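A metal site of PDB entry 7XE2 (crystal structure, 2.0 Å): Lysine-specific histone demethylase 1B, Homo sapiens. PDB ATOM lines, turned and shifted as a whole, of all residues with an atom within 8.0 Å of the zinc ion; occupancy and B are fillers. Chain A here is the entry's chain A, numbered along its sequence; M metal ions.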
ATOM      1  N   GLN A 112      -3.592  17.525  22.123  1.00  0.00           N
ATOM      2  CA  GLN A 112      -3.054  16.616  21.120  1.00  0.00           C
ATOM      3  C   GLN A 112      -1.742  16.000  21.575  1.00  0.00           C
ATOM      4  O   GLN A 112      -0.851  16.704  22.084  1.00  0.00           O
ATOM      5  CB  GLN A 112      -2.794  17.336  19.798  1.00  0.00           C
ATOM      6  CG  GLN A 112      -3.993  17.833  19.082  1.00  0.00           C
ATOM      7  CD  GLN A 112      -3.622  18.983  18.153  1.00  0.00           C
ATOM      8  OE1 GLN A 112      -3.152  20.042  18.597  1.00  0.00           O
ATOM      9  NE2 GLN A 112      -3.837  18.778  16.853  1.00  0.00           N
ATOM     10  N   CYS A 113      -1.606  14.698  21.339  1.00  0.00           N
ATOM     11  CA  CYS A 113      -0.302  14.050  21.452  1.00  0.00           C
ATOM     12  C   CYS A 113       0.705  14.782  20.575  1.00  0.00           C
ATOM     13  O   CYS A 113       0.427  15.120  19.424  1.00  0.00           O
ATOM     14  CB  CYS A 113      -0.392  12.583  21.029  1.00  0.00           C
ATOM     15  SG  CYS A 113       1.143  11.663  21.232  1.00  0.00           S
ATOM     16  N   THR A 114       1.889  15.016  21.129  1.00  0.00           N
ATOM     17  CA  THR A 114       2.949  15.720  20.413  1.00  0.00           C
ATOM     18  C   THR A 114       3.912  14.763  19.728  1.00  0.00           C
ATOM     19  O   THR A 114       4.919  15.205  19.160  1.00  0.00           O
ATOM     20  CB  THR A 114       3.693  16.669  21.357  1.00  0.00           C
ATOM     21  OG1 THR A 114       4.306  15.928  22.407  1.00  0.00           O
ATOM     22  CG2 THR A 114       2.715  17.656  21.973  1.00  0.00           C
ATOM     23  N   LYS A 115       3.647  13.471  19.764  1.00  0.00           N
ATOM     24  CA  LYS A 115       4.387  12.532  18.939  1.00  0.00           C
ATOM     25  C   LYS A 115       3.985  12.786  17.488  1.00  0.00           C
ATOM     26  O   LYS A 115       2.791  12.706  17.171  1.00  0.00           O
ATOM     27  CB  LYS A 115       4.090  11.109  19.380  1.00  0.00           C
ATOM     28  CG  LYS A 115       4.945  10.028  18.754  1.00  0.00           C
ATOM     29  CD  LYS A 115       5.013   8.807  19.670  1.00  0.00           C
ATOM     30  CE  LYS A 115       5.105   7.505  18.871  1.00  0.00           C
ATOM     31  NZ  LYS A 115       3.873   7.252  18.044  1.00  0.00           N
ATOM     32  N   PRO A 116       4.912  13.151  16.593  1.00  0.00           N
ATOM     33  CA  PRO A 116       4.485  13.654  15.271  1.00  0.00           C
ATOM     34  C   PRO A 116       3.723  12.635  14.425  1.00  0.00           C
ATOM     35  O   PRO A 116       2.855  13.035  13.640  1.00  0.00           O
ATOM     36  CB  PRO A 116       5.808  14.062  14.606  1.00  0.00           C
ATOM     37  CG  PRO A 116       6.877  13.383  15.379  1.00  0.00           C
ATOM     38  CD  PRO A 116       6.368  13.241  16.773  1.00  0.00           C
ATOM     39  N   GLU A 117       3.996  11.339  14.566  1.00  0.00           N
ATOM     40  CA  GLU A 117       3.218  10.350  13.830  1.00  0.00           C
ATOM     41  C   GLU A 117       1.876  10.032  14.488  1.00  0.00           C
ATOM     42  O   GLU A 117       1.139   9.198  13.961  1.00  0.00           O
ATOM     43  CB  GLU A 117       4.033   9.063  13.665  1.00  0.00           C
ATOM     44  CG  GLU A 117       4.492   8.421  14.973  1.00  0.00           C
ATOM     45  CD  GLU A 117       5.781   9.055  15.537  1.00  0.00           C
ATOM     46  OE1 GLU A 117       6.044  10.240  15.256  1.00  0.00           O
ATOM     47  OE2 GLU A 117       6.520   8.356  16.254  1.00  0.00           O
ATOM     48  N   CYS A 118       1.546  10.672  15.601  1.00  0.00           N
ATOM     49  CA  CYS A 118       0.323  10.346  16.324  1.00  0.00           C
ATOM     50  C   CYS A 118      -0.671  11.496  16.285  1.00  0.00           C
ATOM     51  O   CYS A 118      -1.669  11.434  15.556  1.00  0.00           O
ATOM     52  CB  CYS A 118       0.641   9.967  17.776  1.00  0.00           C
ATOM     53  SG  CYS A 118      -0.835   9.579  18.735  1.00  0.00           S
ATOM     54  N   ARG A 119      -0.417  12.543  17.079  1.00  0.00           N
ATOM     55  CA  ARG A 119      -1.223  13.773  17.062  1.00  0.00           C
ATOM     56  C   ARG A 119      -2.669  13.529  17.478  1.00  0.00           C
ATOM     57  O   ARG A 119      -3.547  14.366  17.201  1.00  0.00           O
ATOM     58  CB  ARG A 119      -1.203  14.444  15.677  1.00  0.00           C
ATOM     59  CG  ARG A 119       0.181  14.721  15.109  1.00  0.00           C
ATOM     60  CD  ARG A 119       0.890  15.785  15.905  1.00  0.00           C
ATOM     61  NE  ARG A 119       0.296  17.105  15.710  1.00  0.00           N
ATOM     62  CZ  ARG A 119       0.215  18.033  16.665  1.00  0.00           C
ATOM     63  NH1 ARG A 119       0.618  17.793  17.906  1.00  0.00           N
ATOM     64  NH2 ARG A 119      -0.273  19.228  16.360  1.00  0.00           N
ATOM     65  N   LYS A 120      -2.973  12.411  18.151  1.00  0.00           N
ATOM     66  CA  LYS A 120      -4.350  12.141  18.528  1.00  0.00           C
ATOM     67  C   LYS A 120      -4.810  13.071  19.647  1.00  0.00           C
ATOM     68  O   LYS A 120      -4.025  13.449  20.529  1.00  0.00           O
ATOM     69  CB  LYS A 120      -4.518  10.671  18.933  1.00  0.00           C
ATOM     70  CG  LYS A 120      -4.492   9.717  17.734  1.00  0.00           C
ATOM     71  CD  LYS A 120      -4.548   8.261  18.154  1.00  0.00           C
ATOM     72  CE  LYS A 120      -4.209   7.353  16.991  1.00  0.00           C
ATOM     73  NZ  LYS A 120      -4.556   5.928  17.300  1.00  0.00           N
ATOM     74  N   TRP A 121      -6.084  13.449  19.604  1.00  0.00           N
ATOM     75  CA  TRP A 121      -6.710  14.245  20.659  1.00  0.00           C
ATOM     76  C   TRP A 121      -7.083  13.392  21.871  1.00  0.00           C
ATOM     77  O   TRP A 121      -7.682  12.321  21.731  1.00  0.00           O
ATOM     78  CB  TRP A 121      -7.976  14.920  20.118  1.00  0.00           C
ATOM     79  CG  TRP A 121      -7.691  16.107  19.237  1.00  0.00           C
ATOM     80  CD1 TRP A 121      -7.676  16.134  17.876  1.00  0.00           C
ATOM     81  CD2 TRP A 121      -7.367  17.418  19.684  1.00  0.00           C
ATOM     82  NE1 TRP A 121      -7.359  17.402  17.440  1.00  0.00           N
ATOM     83  CE2 TRP A 121      -7.182  18.209  18.532  1.00  0.00           C
ATOM     84  CE3 TRP A 121      -7.221  18.007  20.947  1.00  0.00           C
ATOM     85  CZ2 TRP A 121      -6.859  19.561  18.600  1.00  0.00           C
ATOM     86  CZ3 TRP A 121      -6.902  19.338  21.014  1.00  0.00           C
ATOM     87  CH2 TRP A 121      -6.720  20.107  19.851  1.00  0.00           C
ATOM     88  N   ARG A 122      -6.781  13.904  23.067  1.00  0.00           N
ATOM     89  CA  ARG A 122      -7.069  13.211  24.319  1.00  0.00           C
ATOM     90  C   ARG A 122      -7.705  14.157  25.330  1.00  0.00           C
ATOM     91  O   ARG A 122      -7.310  15.325  25.434  1.00  0.00           O
ATOM     92  CB  ARG A 122      -5.795  12.614  24.914  1.00  0.00           C
ATOM     93  CG  ARG A 122      -5.049  11.665  23.998  1.00  0.00           C
ATOM     94  CD  ARG A 122      -5.869  10.384  23.689  1.00  0.00           C
ATOM     95  NE  ARG A 122      -5.049   9.468  22.918  1.00  0.00           N
ATOM     96  CZ  ARG A 122      -5.488   8.414  22.255  1.00  0.00           C
ATOM     97  NH1 ARG A 122      -6.782   8.111  22.225  1.00  0.00           N
ATOM     98  NH2 ARG A 122      -4.614   7.635  21.623  1.00  0.00           N
ATOM     99  N   TYR A 138       2.779  16.986  25.535  1.00  0.00           N
ATOM    100  CA  TYR A 138       1.841  15.926  25.882  1.00  0.00           C
ATOM    101  C   TYR A 138       2.043  14.698  24.990  1.00  0.00           C
ATOM    102  O   TYR A 138       2.310  14.809  23.795  1.00  0.00           O
ATOM    103  CB  TYR A 138       0.394  16.406  25.755  1.00  0.00           C
ATOM    104  CG  TYR A 138      -0.599  15.323  26.108  1.00  0.00           C
ATOM    105  CD1 TYR A 138      -0.845  14.996  27.436  1.00  0.00           C
ATOM    106  CD2 TYR A 138      -1.272  14.613  25.118  1.00  0.00           C
ATOM    107  CE1 TYR A 138      -1.734  13.999  27.777  1.00  0.00           C
ATOM    108  CE2 TYR A 138      -2.179  13.592  25.457  1.00  0.00           C
ATOM    109  CZ  TYR A 138      -2.401  13.297  26.787  1.00  0.00           C
ATOM    110  OH  TYR A 138      -3.278  12.315  27.149  1.00  0.00           O
ATOM    111  N   ARG A 139       1.926  13.527  25.610  1.00  0.00           N
ATOM    112  CA  ARG A 139       1.981  12.260  24.900  1.00  0.00           C
ATOM    113  C   ARG A 139       0.907  11.338  25.466  1.00  0.00           C
ATOM    114  O   ARG A 139       0.708  11.299  26.688  1.00  0.00           O
ATOM    115  CB  ARG A 139       3.371  11.609  25.027  1.00  0.00           C
ATOM    116  CG  ARG A 139       4.459  12.483  24.440  1.00  0.00           C
ATOM    117  CD  ARG A 139       5.447  11.668  23.631  1.00  0.00           C
ATOM    118  NE  ARG A 139       6.296  12.541  22.822  1.00  0.00           N
ATOM    119  CZ  ARG A 139       7.276  12.109  22.038  1.00  0.00           C
ATOM    120  NH1 ARG A 139       7.541  10.814  21.908  1.00  0.00           N
ATOM    121  NH2 ARG A 139       7.996  12.996  21.365  1.00  0.00           N
ATOM    122  N   CYS A 140       0.208  10.629  24.575  1.00  0.00           N
ATOM    123  CA  CYS A 140      -0.825   9.675  24.961  1.00  0.00           C
ATOM    124  C   CYS A 140      -0.373   8.810  26.129  1.00  0.00           C
ATOM    125  O   CYS A 140       0.732   8.261  26.127  1.00  0.00           O
ATOM    126  CB  CYS A 140      -1.178   8.771  23.777  1.00  0.00           C
ATOM    127  SG  CYS A 140      -1.748   9.625  22.302  1.00  0.00           S
ATOM    128  N   GLY A 141      -1.229   8.735  27.149  1.00  0.00           N
ATOM    129  CA  GLY A 141      -0.979   7.852  28.277  1.00  0.00           C
ATOM    130  C   GLY A 141      -0.022   8.375  29.333  1.00  0.00           C
ATOM    131  O   GLY A 141       0.177   7.703  30.347  1.00  0.00           O
ATOM    132  N   THR A 152       6.596   4.269  26.984  1.00  0.00           N
ATOM    133  CA  THR A 152       6.620   3.719  25.631  1.00  0.00           C
ATOM    134  C   THR A 152       5.700   4.523  24.710  1.00  0.00           C
ATOM    135  O   THR A 152       5.602   5.740  24.834  1.00  0.00           O
ATOM    136  CB  THR A 152       6.210   2.239  25.624  1.00  0.00           C
ATOM    137  OG1 THR A 152       4.808   2.098  25.905  1.00  0.00           O
ATOM    138  CG2 THR A 152       7.014   1.466  26.661  1.00  0.00           C
ATOM    139  N   SER A 153       5.029   3.833  23.780  1.00  0.00           N
ATOM    140  CA  SER A 153       4.039   4.483  22.920  1.00  0.00           C
ATOM    141  C   SER A 153       2.859   3.554  22.649  1.00  0.00           C
ATOM    142  O   SER A 153       2.179   3.686  21.632  1.00  0.00           O
ATOM    143  CB  SER A 153       4.656   4.929  21.593  1.00  0.00           C
ATOM    144  OG  SER A 153       5.509   6.053  21.777  1.00  0.00           O
ATOM    145  N   ASP A 154       2.606   2.606  23.552  1.00  0.00           N
ATOM    146  CA  ASP A 154       1.493   1.669  23.364  1.00  0.00           C
ATOM    147  C   ASP A 154       0.149   2.383  23.452  1.00  0.00           C
ATOM    148  O   ASP A 154      -0.806   1.969  22.771  1.00  0.00           O
ATOM    149  CB  ASP A 154       1.571   0.545  24.405  1.00  0.00           C
ATOM    150  CG  ASP A 154       0.858  -0.730  23.941  1.00  0.00           C
ATOM    151  OD1 ASP A 154       0.376  -0.754  22.786  1.00  0.00           O
ATOM    152  OD2 ASP A 154       0.781  -1.716  24.720  1.00  0.00           O
ATOM    153  N   HIS A 155       0.052   3.435  24.261  1.00  0.00           N
ATOM    154  CA  HIS A 155      -1.194   4.181  24.425  1.00  0.00           C
ATOM    155  C   HIS A 155      -1.547   5.026  23.200  1.00  0.00           C
ATOM    156  O   HIS A 155      -2.706   5.437  23.064  1.00  0.00           O
ATOM    157  CB  HIS A 155      -1.109   5.099  25.647  1.00  0.00           C
ATOM    158  CG  HIS A 155      -1.023   4.367  26.944  1.00  0.00           C
ATOM    159  ND1 HIS A 155       0.035   3.552  27.270  1.00  0.00           N
ATOM    160  CD2 HIS A 155      -1.870   4.321  28.006  1.00  0.00           C
ATOM    161  CE1 HIS A 155      -0.158   3.029  28.473  1.00  0.00           C
ATOM    162  NE2 HIS A 155      -1.303   3.485  28.940  1.00  0.00           N
ATOM    163  N   CYS A 156      -0.577   5.317  22.324  1.00  0.00           N
ATOM    164  CA  CYS A 156      -0.888   6.102  21.129  1.00  0.00           C
ATOM    165  C   CYS A 156      -1.837   5.347  20.194  1.00  0.00           C
ATOM    166  O   CYS A 156      -2.661   5.970  19.521  1.00  0.00           O
ATOM    167  CB  CYS A 156       0.386   6.478  20.380  1.00  0.00           C
ATOM    168  SG  CYS A 156       1.438   7.741  21.229  1.00  0.00           S
ATOM    169  N   SER A 157      -1.753   4.032  20.176  1.00  0.00           N
ATOM    170  CA  SER A 157      -2.556   3.253  19.237  1.00  0.00           C
ATOM    171  C   SER A 157      -4.039   3.270  19.581  1.00  0.00           C
ATOM    172  O   SER A 157      -4.845   2.881  18.728  1.00  0.00           O
ATOM    173  CB  SER A 157      -2.069   1.805  19.201  1.00  0.00           C
ATOM    174  OG  SER A 157      -0.828   1.746  18.524  1.00  0.00           O
ATOM    175  N   LEU A 158      -4.394   3.668  20.803  1.00  0.00           N
ATOM    176  CA  LEU A 158      -5.782   3.595  21.209  1.00  0.00           C
ATOM    177  C   LEU A 158      -6.596   4.588  20.380  1.00  0.00           C
ATOM    178  O   LEU A 158      -6.107   5.689  20.075  1.00  0.00           O
ATOM    179  CB  LEU A 158      -5.947   3.901  22.706  1.00  0.00           C
ATOM    180  CG  LEU A 158      -5.430   2.871  23.710  1.00  0.00           C
ATOM    181  CD1 LEU A 158      -5.716   3.313  25.147  1.00  0.00           C
ATOM    182  CD2 LEU A 158      -5.991   1.436  23.477  1.00  0.00           C
HETATM  183 ZN    ZN M   1       0.022   9.582  20.858  1.00  0.00          ZN
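The guanidinium group of Arg 122 is in hydrogen-bond range of the backbone carbonyl oxygen of Cys 156, 3.3 Å away. NH1 of Arg 119 lies within hydrogen-bond range of O of Cys 113, at 3.1 Å. SG of Cys 113 lies close to N of Lys 115 (3.4 Å). NE of Arg 122 lies close to SG of Cys 140 (3.4 Å). O of Lys 120 is in hydrogen-bond range of N of Cys 113. The backbone carbonyl oxygen of Cys 156 lies within hydrogen-bond range of the side-chain amino group of Lys 120. SG of Cys 118 sits close to N of Lys 120.
Within 4 Å of the zinc ion: Cys 113, Cys 118, Cys 140 and Cys 156.
The zinc ion is bound by the side-chain sulfur of Cys 140 (2.3 Å), the side-chain sulfur of Cys 118 (2.3 Å), the side-chain sulfur of Cys 156 (2.4 Å) and the side-chain sulfur of Cys 113 (2.4 Å).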
